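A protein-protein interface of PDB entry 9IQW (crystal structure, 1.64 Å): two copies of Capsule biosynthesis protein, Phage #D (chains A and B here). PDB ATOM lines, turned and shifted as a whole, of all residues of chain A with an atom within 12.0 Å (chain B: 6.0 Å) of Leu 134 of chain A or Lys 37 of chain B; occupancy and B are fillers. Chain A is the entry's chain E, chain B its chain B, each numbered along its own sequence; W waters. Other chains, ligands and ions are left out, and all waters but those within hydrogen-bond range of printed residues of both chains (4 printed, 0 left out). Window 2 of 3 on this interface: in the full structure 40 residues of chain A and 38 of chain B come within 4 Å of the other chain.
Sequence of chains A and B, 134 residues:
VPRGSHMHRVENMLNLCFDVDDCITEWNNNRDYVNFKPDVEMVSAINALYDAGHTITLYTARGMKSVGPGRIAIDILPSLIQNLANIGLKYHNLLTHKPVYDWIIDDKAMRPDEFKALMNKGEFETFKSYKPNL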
ATOM      1  N   SER A 129      -4.632  21.907   6.156  1.00  0.00           N
ATOM      2  CA  SER A 129      -5.933  21.891   6.800  1.00  0.00           C
ATOM      3  C   SER A 129      -7.042  21.615   5.783  1.00  0.00           C
ATOM      4  O   SER A 129      -6.812  21.590   4.572  1.00  0.00           O
ATOM      5  CB  SER A 129      -6.169  23.198   7.545  1.00  0.00           C
ATOM      6  OG  SER A 129      -6.093  24.314   6.687  1.00  0.00           O
ATOM      7  N   TYR A 130      -8.257  21.405   6.296  1.00  0.00           N
ATOM      8  CA  TYR A 130      -9.383  21.018   5.467  1.00  0.00           C
ATOM      9  C   TYR A 130      -9.908  22.170   4.620  1.00  0.00           C
ATOM     10  O   TYR A 130     -10.020  23.296   5.103  1.00  0.00           O
ATOM     11  CB  TYR A 130     -10.506  20.464   6.345  1.00  0.00           C
ATOM     12  CG  TYR A 130     -11.808  20.293   5.606  1.00  0.00           C
ATOM     13  CD1 TYR A 130     -12.108  19.108   4.944  1.00  0.00           C
ATOM     14  CD2 TYR A 130     -12.744  21.316   5.560  1.00  0.00           C
ATOM     15  CE1 TYR A 130     -13.306  18.949   4.260  1.00  0.00           C
ATOM     16  CE2 TYR A 130     -13.939  21.168   4.883  1.00  0.00           C
ATOM     17  CZ  TYR A 130     -14.225  19.975   4.241  1.00  0.00           C
ATOM     18  OH  TYR A 130     -15.408  19.819   3.568  1.00  0.00           O
ATOM     19  N   LYS A 131     -10.230  21.854   3.361  1.00  0.00           N
ATOM     20  CA  LYS A 131     -10.927  22.778   2.484  1.00  0.00           C
ATOM     21  C   LYS A 131     -12.101  22.039   1.849  1.00  0.00           C
ATOM     22  O   LYS A 131     -11.974  20.868   1.482  1.00  0.00           O
ATOM     23  CB  LYS A 131     -10.020  23.327   1.373  1.00  0.00           C
ATOM     24  CG  LYS A 131      -8.764  24.039   1.856  1.00  0.00           C
ATOM     25  CD  LYS A 131      -9.042  25.334   2.613  1.00  0.00           C
ATOM     26  CE  LYS A 131      -7.745  25.978   3.054  1.00  0.00           C
ATOM     27  NZ  LYS A 131      -7.971  27.051   4.055  1.00  0.00           N
ATOM     28  N   PRO A 132     -13.279  22.689   1.719  1.00  0.00           N
ATOM     29  CA  PRO A 132     -14.427  22.059   1.076  1.00  0.00           C
ATOM     30  C   PRO A 132     -14.165  21.563  -0.343  1.00  0.00           C
ATOM     31  O   PRO A 132     -14.704  20.531  -0.737  1.00  0.00           O
ATOM     32  CB  PRO A 132     -15.477  23.168   1.104  1.00  0.00           C
ATOM     33  CG  PRO A 132     -15.094  24.038   2.235  1.00  0.00           C
ATOM     34  CD  PRO A 132     -13.601  24.010   2.283  1.00  0.00           C
ATOM     35  N   ASN A 133     -13.374  22.317  -1.116  1.00  0.00           N
ATOM     36  CA  ASN A 133     -13.096  21.957  -2.502  1.00  0.00           C
ATOM     37  C   ASN A 133     -14.375  21.577  -3.253  1.00  0.00           C
ATOM     38  O   ASN A 133     -14.471  20.502  -3.843  1.00  0.00           O
ATOM     39  CB  ASN A 133     -12.093  20.796  -2.565  1.00  0.00           C
ATOM     40  CG  ASN A 133     -10.692  21.159  -2.126  1.00  0.00           C
ATOM     41  OD1 ASN A 133     -10.130  22.202  -2.510  1.00  0.00           O
ATOM     42  ND2 ASN A 133     -10.104  20.318  -1.288  1.00  0.00           N
ATOM     43  N   LEU A 134     -15.358  22.481  -3.239  1.00  0.00           N
ATOM     44  CA  LEU A 134     -16.658  22.208  -3.828  1.00  0.00           C
ATOM     45  C   LEU A 134     -16.594  22.273  -5.337  1.00  0.00           C
ATOM     46  O   LEU A 134     -15.742  22.974  -5.917  1.00  0.00           O
ATOM     47  CB  LEU A 134     -17.704  23.224  -3.312  1.00  0.00           C
ATOM     48  CG  LEU A 134     -17.929  23.228  -1.802  1.00  0.00           C
ATOM     49  CD1 LEU A 134     -18.993  24.209  -1.415  1.00  0.00           C
ATOM     50  CD2 LEU A 134     -18.286  21.851  -1.272  1.00  0.00           C
ATOM     51  OXT LEU A 134     -17.436  21.642  -5.985  1.00  0.00           O
ATOM     52  N   ILE B  24     -19.108  24.760   6.846  1.00  0.00           N
ATOM     53  CA  ILE B  24     -20.473  24.700   6.339  1.00  0.00           C
ATOM     54  C   ILE B  24     -20.573  25.312   4.946  1.00  0.00           C
ATOM     55  O   ILE B  24     -21.266  24.770   4.082  1.00  0.00           O
ATOM     56  CB  ILE B  24     -21.420  25.382   7.330  1.00  0.00           C
ATOM     57  CG1 ILE B  24     -21.385  24.683   8.699  1.00  0.00           C
ATOM     58  CG2 ILE B  24     -22.853  25.446   6.758  1.00  0.00           C
ATOM     59  CD1 ILE B  24     -22.131  25.427   9.773  1.00  0.00           C
ATOM     60  N   THR B  25     -19.893  26.444   4.742  1.00  0.00           N
ATOM     61  CA  THR B  25     -19.776  27.087   3.445  1.00  0.00           C
ATOM     62  C   THR B  25     -18.311  27.197   3.045  1.00  0.00           C
ATOM     63  O   THR B  25     -17.415  26.957   3.856  1.00  0.00           O
ATOM     64  CB  THR B  25     -20.453  28.475   3.449  1.00  0.00           C
ATOM     65  OG1 THR B  25     -19.845  29.335   4.432  1.00  0.00           O
ATOM     66  CG2 THR B  25     -21.946  28.380   3.731  1.00  0.00           C
ATOM     67  N   GLU B  26     -18.083  27.519   1.770  1.00  0.00           N
ATOM     68  CA  GLU B  26     -16.749  27.635   1.210  1.00  0.00           C
ATOM     69  C   GLU B  26     -16.348  29.108   1.163  1.00  0.00           C
ATOM     70  O   GLU B  26     -17.149  29.973   0.793  1.00  0.00           O
ATOM     71  CB  GLU B  26     -16.724  27.020  -0.188  1.00  0.00           C
ATOM     72  CG  GLU B  26     -15.391  27.078  -0.922  1.00  0.00           C
ATOM     73  CD  GLU B  26     -15.409  26.298  -2.213  1.00  0.00           C
ATOM     74  OE1 GLU B  26     -16.218  26.636  -3.107  1.00  0.00           O
ATOM     75  OE2 GLU B  26     -14.634  25.319  -2.318  1.00  0.00           O
ATOM     76  N   ASN B  35     -23.477  35.315  -0.733  1.00  0.00           N
ATOM     77  CA  ASN B  35     -23.417  34.305  -1.780  1.00  0.00           C
ATOM     78  C   ASN B  35     -22.380  33.200  -1.595  1.00  0.00           C
ATOM     79  O   ASN B  35     -22.143  32.420  -2.518  1.00  0.00           O
ATOM     80  CB  ASN B  35     -23.224  34.958  -3.122  1.00  0.00           C
ATOM     81  CG  ASN B  35     -24.476  35.672  -3.562  1.00  0.00           C
ATOM     82  OD1 ASN B  35     -25.577  35.119  -3.481  1.00  0.00           O
ATOM     83  ND2 ASN B  35     -24.340  36.920  -3.986  1.00  0.00           N
ATOM     84  N   PHE B  36     -21.820  33.080  -0.385  1.00  0.00           N
ATOM     85  CA  PHE B  36     -20.952  31.958  -0.079  1.00  0.00           C
ATOM     86  C   PHE B  36     -21.702  30.655  -0.330  1.00  0.00           C
ATOM     87  O   PHE B  36     -22.873  30.520   0.028  1.00  0.00           O
ATOM     88  CB  PHE B  36     -20.445  32.032   1.374  1.00  0.00           C
ATOM     89  CG  PHE B  36     -19.257  32.940   1.642  1.00  0.00           C
ATOM     90  CD1 PHE B  36     -18.709  33.722   0.636  1.00  0.00           C
ATOM     91  CD2 PHE B  36     -18.666  32.973   2.887  1.00  0.00           C
ATOM     92  CE1 PHE B  36     -17.600  34.528   0.885  1.00  0.00           C
ATOM     93  CE2 PHE B  36     -17.574  33.782   3.130  1.00  0.00           C
ATOM     94  CZ  PHE B  36     -17.031  34.542   2.118  1.00  0.00           C
ATOM     95  N   LYS B  37     -20.996  29.708  -0.952  1.00  0.00           N
ATOM     96  CA  LYS B  37     -21.594  28.465  -1.415  1.00  0.00           C
ATOM     97  C   LYS B  37     -21.629  27.435  -0.296  1.00  0.00           C
ATOM     98  O   LYS B  37     -20.616  27.199   0.365  1.00  0.00           O
ATOM     99  CB  LYS B  37     -20.792  27.911  -2.611  1.00  0.00           C
ATOM    100  CG  LYS B  37     -21.287  26.571  -3.107  1.00  0.00           C
ATOM    101  CD  LYS B  37     -20.229  25.717  -3.799  1.00  0.00           C
ATOM    102  CE  LYS B  37     -20.679  25.310  -5.191  1.00  0.00           C
ATOM    103  NZ  LYS B  37     -21.984  24.567  -5.184  1.00  0.00           N
ATOM    104  N   PRO B  38     -22.786  26.782  -0.043  1.00  0.00           N
ATOM    105  CA  PRO B  38     -22.859  25.739   0.968  1.00  0.00           C
ATOM    106  C   PRO B  38     -22.302  24.403   0.497  1.00  0.00           C
ATOM    107  O   PRO B  38     -22.431  24.041  -0.676  1.00  0.00           O
ATOM    108  CB  PRO B  38     -24.350  25.659   1.240  1.00  0.00           C
ATOM    109  CG  PRO B  38     -24.980  25.961  -0.096  1.00  0.00           C
ATOM    110  CD  PRO B  38     -24.087  27.034  -0.683  1.00  0.00           C
ATOM    111  N   ASP B  39     -21.696  23.682   1.449  1.00  0.00           N
ATOM    112  CA  ASP B  39     -21.482  22.255   1.317  1.00  0.00           C
ATOM    113  C   ASP B  39     -22.815  21.617   1.700  1.00  0.00           C
ATOM    114  O   ASP B  39     -23.179  21.566   2.877  1.00  0.00           O
ATOM    115  CB  ASP B  39     -20.346  21.822   2.230  1.00  0.00           C
ATOM    116  CG  ASP B  39     -20.026  20.348   2.179  1.00  0.00           C
ATOM    117  OD1 ASP B  39     -20.892  19.572   1.721  1.00  0.00           O
ATOM    118  OD2 ASP B  39     -18.889  19.985   2.549  1.00  0.00           O
ATOM    119  N   VAL B  40     -23.584  21.188   0.694  1.00  0.00           N
ATOM    120  CA  VAL B  40     -24.937  20.715   0.939  1.00  0.00           C
ATOM    121  C   VAL B  40     -24.946  19.467   1.817  1.00  0.00           C
ATOM    122  O   VAL B  40     -25.914  19.228   2.527  1.00  0.00           O
ATOM    123  CB  VAL B  40     -25.737  20.502  -0.359  1.00  0.00           C
ATOM    124  CG1 VAL B  40     -25.915  21.828  -1.089  1.00  0.00           C
ATOM    125  CG2 VAL B  40     -25.111  19.439  -1.256  1.00  0.00           C
ATOM    126  N   ASN B  83     -27.263  34.401   4.659  1.00  0.00           N
ATOM    127  CA  ASN B  83     -26.698  33.251   3.960  1.00  0.00           C
ATOM    128  C   ASN B  83     -27.204  31.939   4.562  1.00  0.00           C
ATOM    129  O   ASN B  83     -27.645  31.049   3.843  1.00  0.00           O
ATOM    130  CB  ASN B  83     -25.190  33.301   3.988  1.00  0.00           C
ATOM    131  CG  ASN B  83     -24.528  32.093   3.372  1.00  0.00           C
ATOM    132  OD1 ASN B  83     -24.386  32.003   2.163  1.00  0.00           O
ATOM    133  ND2 ASN B  83     -24.104  31.169   4.180  1.00  0.00           N
ATOM    134  N   ILE B  87     -29.496  29.063   2.663  1.00  0.00           N
ATOM    135  CA  ILE B  87     -29.045  27.693   2.449  1.00  0.00           C
ATOM    136  C   ILE B  87     -29.909  26.688   3.215  1.00  0.00           C
ATOM    137  O   ILE B  87     -29.779  25.486   2.987  1.00  0.00           O
ATOM    138  CB  ILE B  87     -27.538  27.486   2.750  1.00  0.00           C
ATOM    139  CG1 ILE B  87     -27.258  27.496   4.241  1.00  0.00           C
ATOM    140  CG2 ILE B  87     -26.676  28.524   2.012  1.00  0.00           C
ATOM    141  CD1 ILE B  87     -25.744  27.477   4.622  1.00  0.00           C
ATOM    142  N   LYS B 116     -18.338  14.337   8.051  1.00  0.00           N
ATOM    143  CA  LYS B 116     -19.191  13.855   6.972  1.00  0.00           C
ATOM    144  C   LYS B 116     -19.103  12.337   6.798  1.00  0.00           C
ATOM    145  O   LYS B 116     -20.115  11.683   6.561  1.00  0.00           O
ATOM    146  CB  LYS B 116     -18.844  14.559   5.653  1.00  0.00           C
ATOM    147  CG  LYS B 116     -19.352  15.974   5.599  1.00  0.00           C
ATOM    148  CD  LYS B 116     -19.097  16.644   4.272  1.00  0.00           C
ATOM    149  CE  LYS B 116     -17.663  17.082   4.110  1.00  0.00           C
ATOM    150  NZ  LYS B 116     -17.428  17.638   2.750  1.00  0.00           N
HETATM  151  O   HOH W   1     -16.380  18.469   0.164  1.00  0.00           O
HETATM  152  O   HOH W   2     -12.318  25.013  -0.960  1.00  0.00           O
HETATM  153  O   HOH W   3     -16.130  25.771  -5.519  1.00  0.00           O
HETATM  154  O   HOH W   4     -17.201  21.437   3.809  1.00  0.00           O
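Leu 134 of chain A touches just these residues of chain B: Glu 26, Lys 37, Pro 38 and Asp 39. Lys 37 of chain B touches just one residue of chain A: Leu 134. No residue of chain A comes within 4 Å of Thr 25 of chain B. Of chain A, only Asn 133 and Leu 134 come within 4 Å of Glu 26 of chain B. No residue of chain A comes within 4 Å of Phe 36 of chain B. Pro 38 of chain B touches just one residue of chain A: Leu 134 (3.5 Å). Asp 39 of chain B touches just these residues of chain A: Tyr 130 and Leu 134. Of the printed residues of chain B, Tyr 130 of chain A touches Asp 39 and Lys 116. Of the printed residues of chain B, Asn 133 of chain A touches Glu 26 (3.5 Å).
Printed residues of chain B that touch a printed residue of chain A: Glu 26, Lys 37, Pro 38, Asp 39 and Lys 116. Along chain A the printed residues that touch a printed residue of chain B span positions 130 to 134. Among the printed residues, 7 pairs touch across the chains. Among the printed residues, no Asp or Glu carboxylate lies within 4 Å of a Lys or Arg side-chain nitrogen of the other chain.
Water W4 bridges the side-chain hydroxyl of Tyr 130 of chain A and the side-chain carboxylate of Asp 39 of chain B. Water W3 bridges the side-chain carboxylate (OE1) of Glu 26 of chain B (2.6 Å) and the chain-end carboxylate (O) of Leu 134 of chain A (2.9 Å). Water W2 lies within hydrogen-bond range of the side-chain carboxylate (OE2) of Glu 26 of chain B (2.7 Å) and the backbone NH (N) of Asn 133 of chain A (2.9 Å). Water W1 lies within hydrogen-bond range of O of Pro 132 of chain A and NZ of Lys 116 of chain B.
No position is printed for both chains.
The backbone carbonyl oxygen (O) of Ile 24 of chain B lies within hydrogen-bond range of the backbone NH (N) of Asp 39 of chain B, 2.9 Å away. The backbone NH of Glu 26 of chain B lies within hydrogen-bond range of the backbone carbonyl oxygen of Lys 37 of chain B (2.9 Å). The side-chain amino group of Lys 116 of chain B lies within salt-bridge range of the side-chain carboxylate of Asp 39 of chain B (2.8 Å). O of Lys 131 of chain A lies within hydrogen-bond range of ND2 of Asn 133 of chain A (3.4 Å).
OE2 of Glu 26 of chain B is in hydrogen-bond range of N of Asn 133 of chain A, at 3.5 Å. The side-chain carboxylate (OE2) of Glu 26 of chain B is in hydrogen-bond range of the backbone NH (N) of Leu 134 of chain A, at 3.1 Å. The side-chain amino group (NZ) of Lys 116 of chain B is in hydrogen-bond range of the side-chain hydroxyl (OH) of Tyr 130 of chain A (3.1 Å).
Among the printed residues, pairs that only touch across the chains: Tyr 130 of chain A with Asp 39 of chain B (3.6 Å), Leu 134 of chain A with Lys 37 of chain B (3.1 Å), Leu 134 of chain A with Pro 38 of chain B (3.5 Å) and Leu 134 of chain A with Asp 39 of chain B (3.97 Å).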
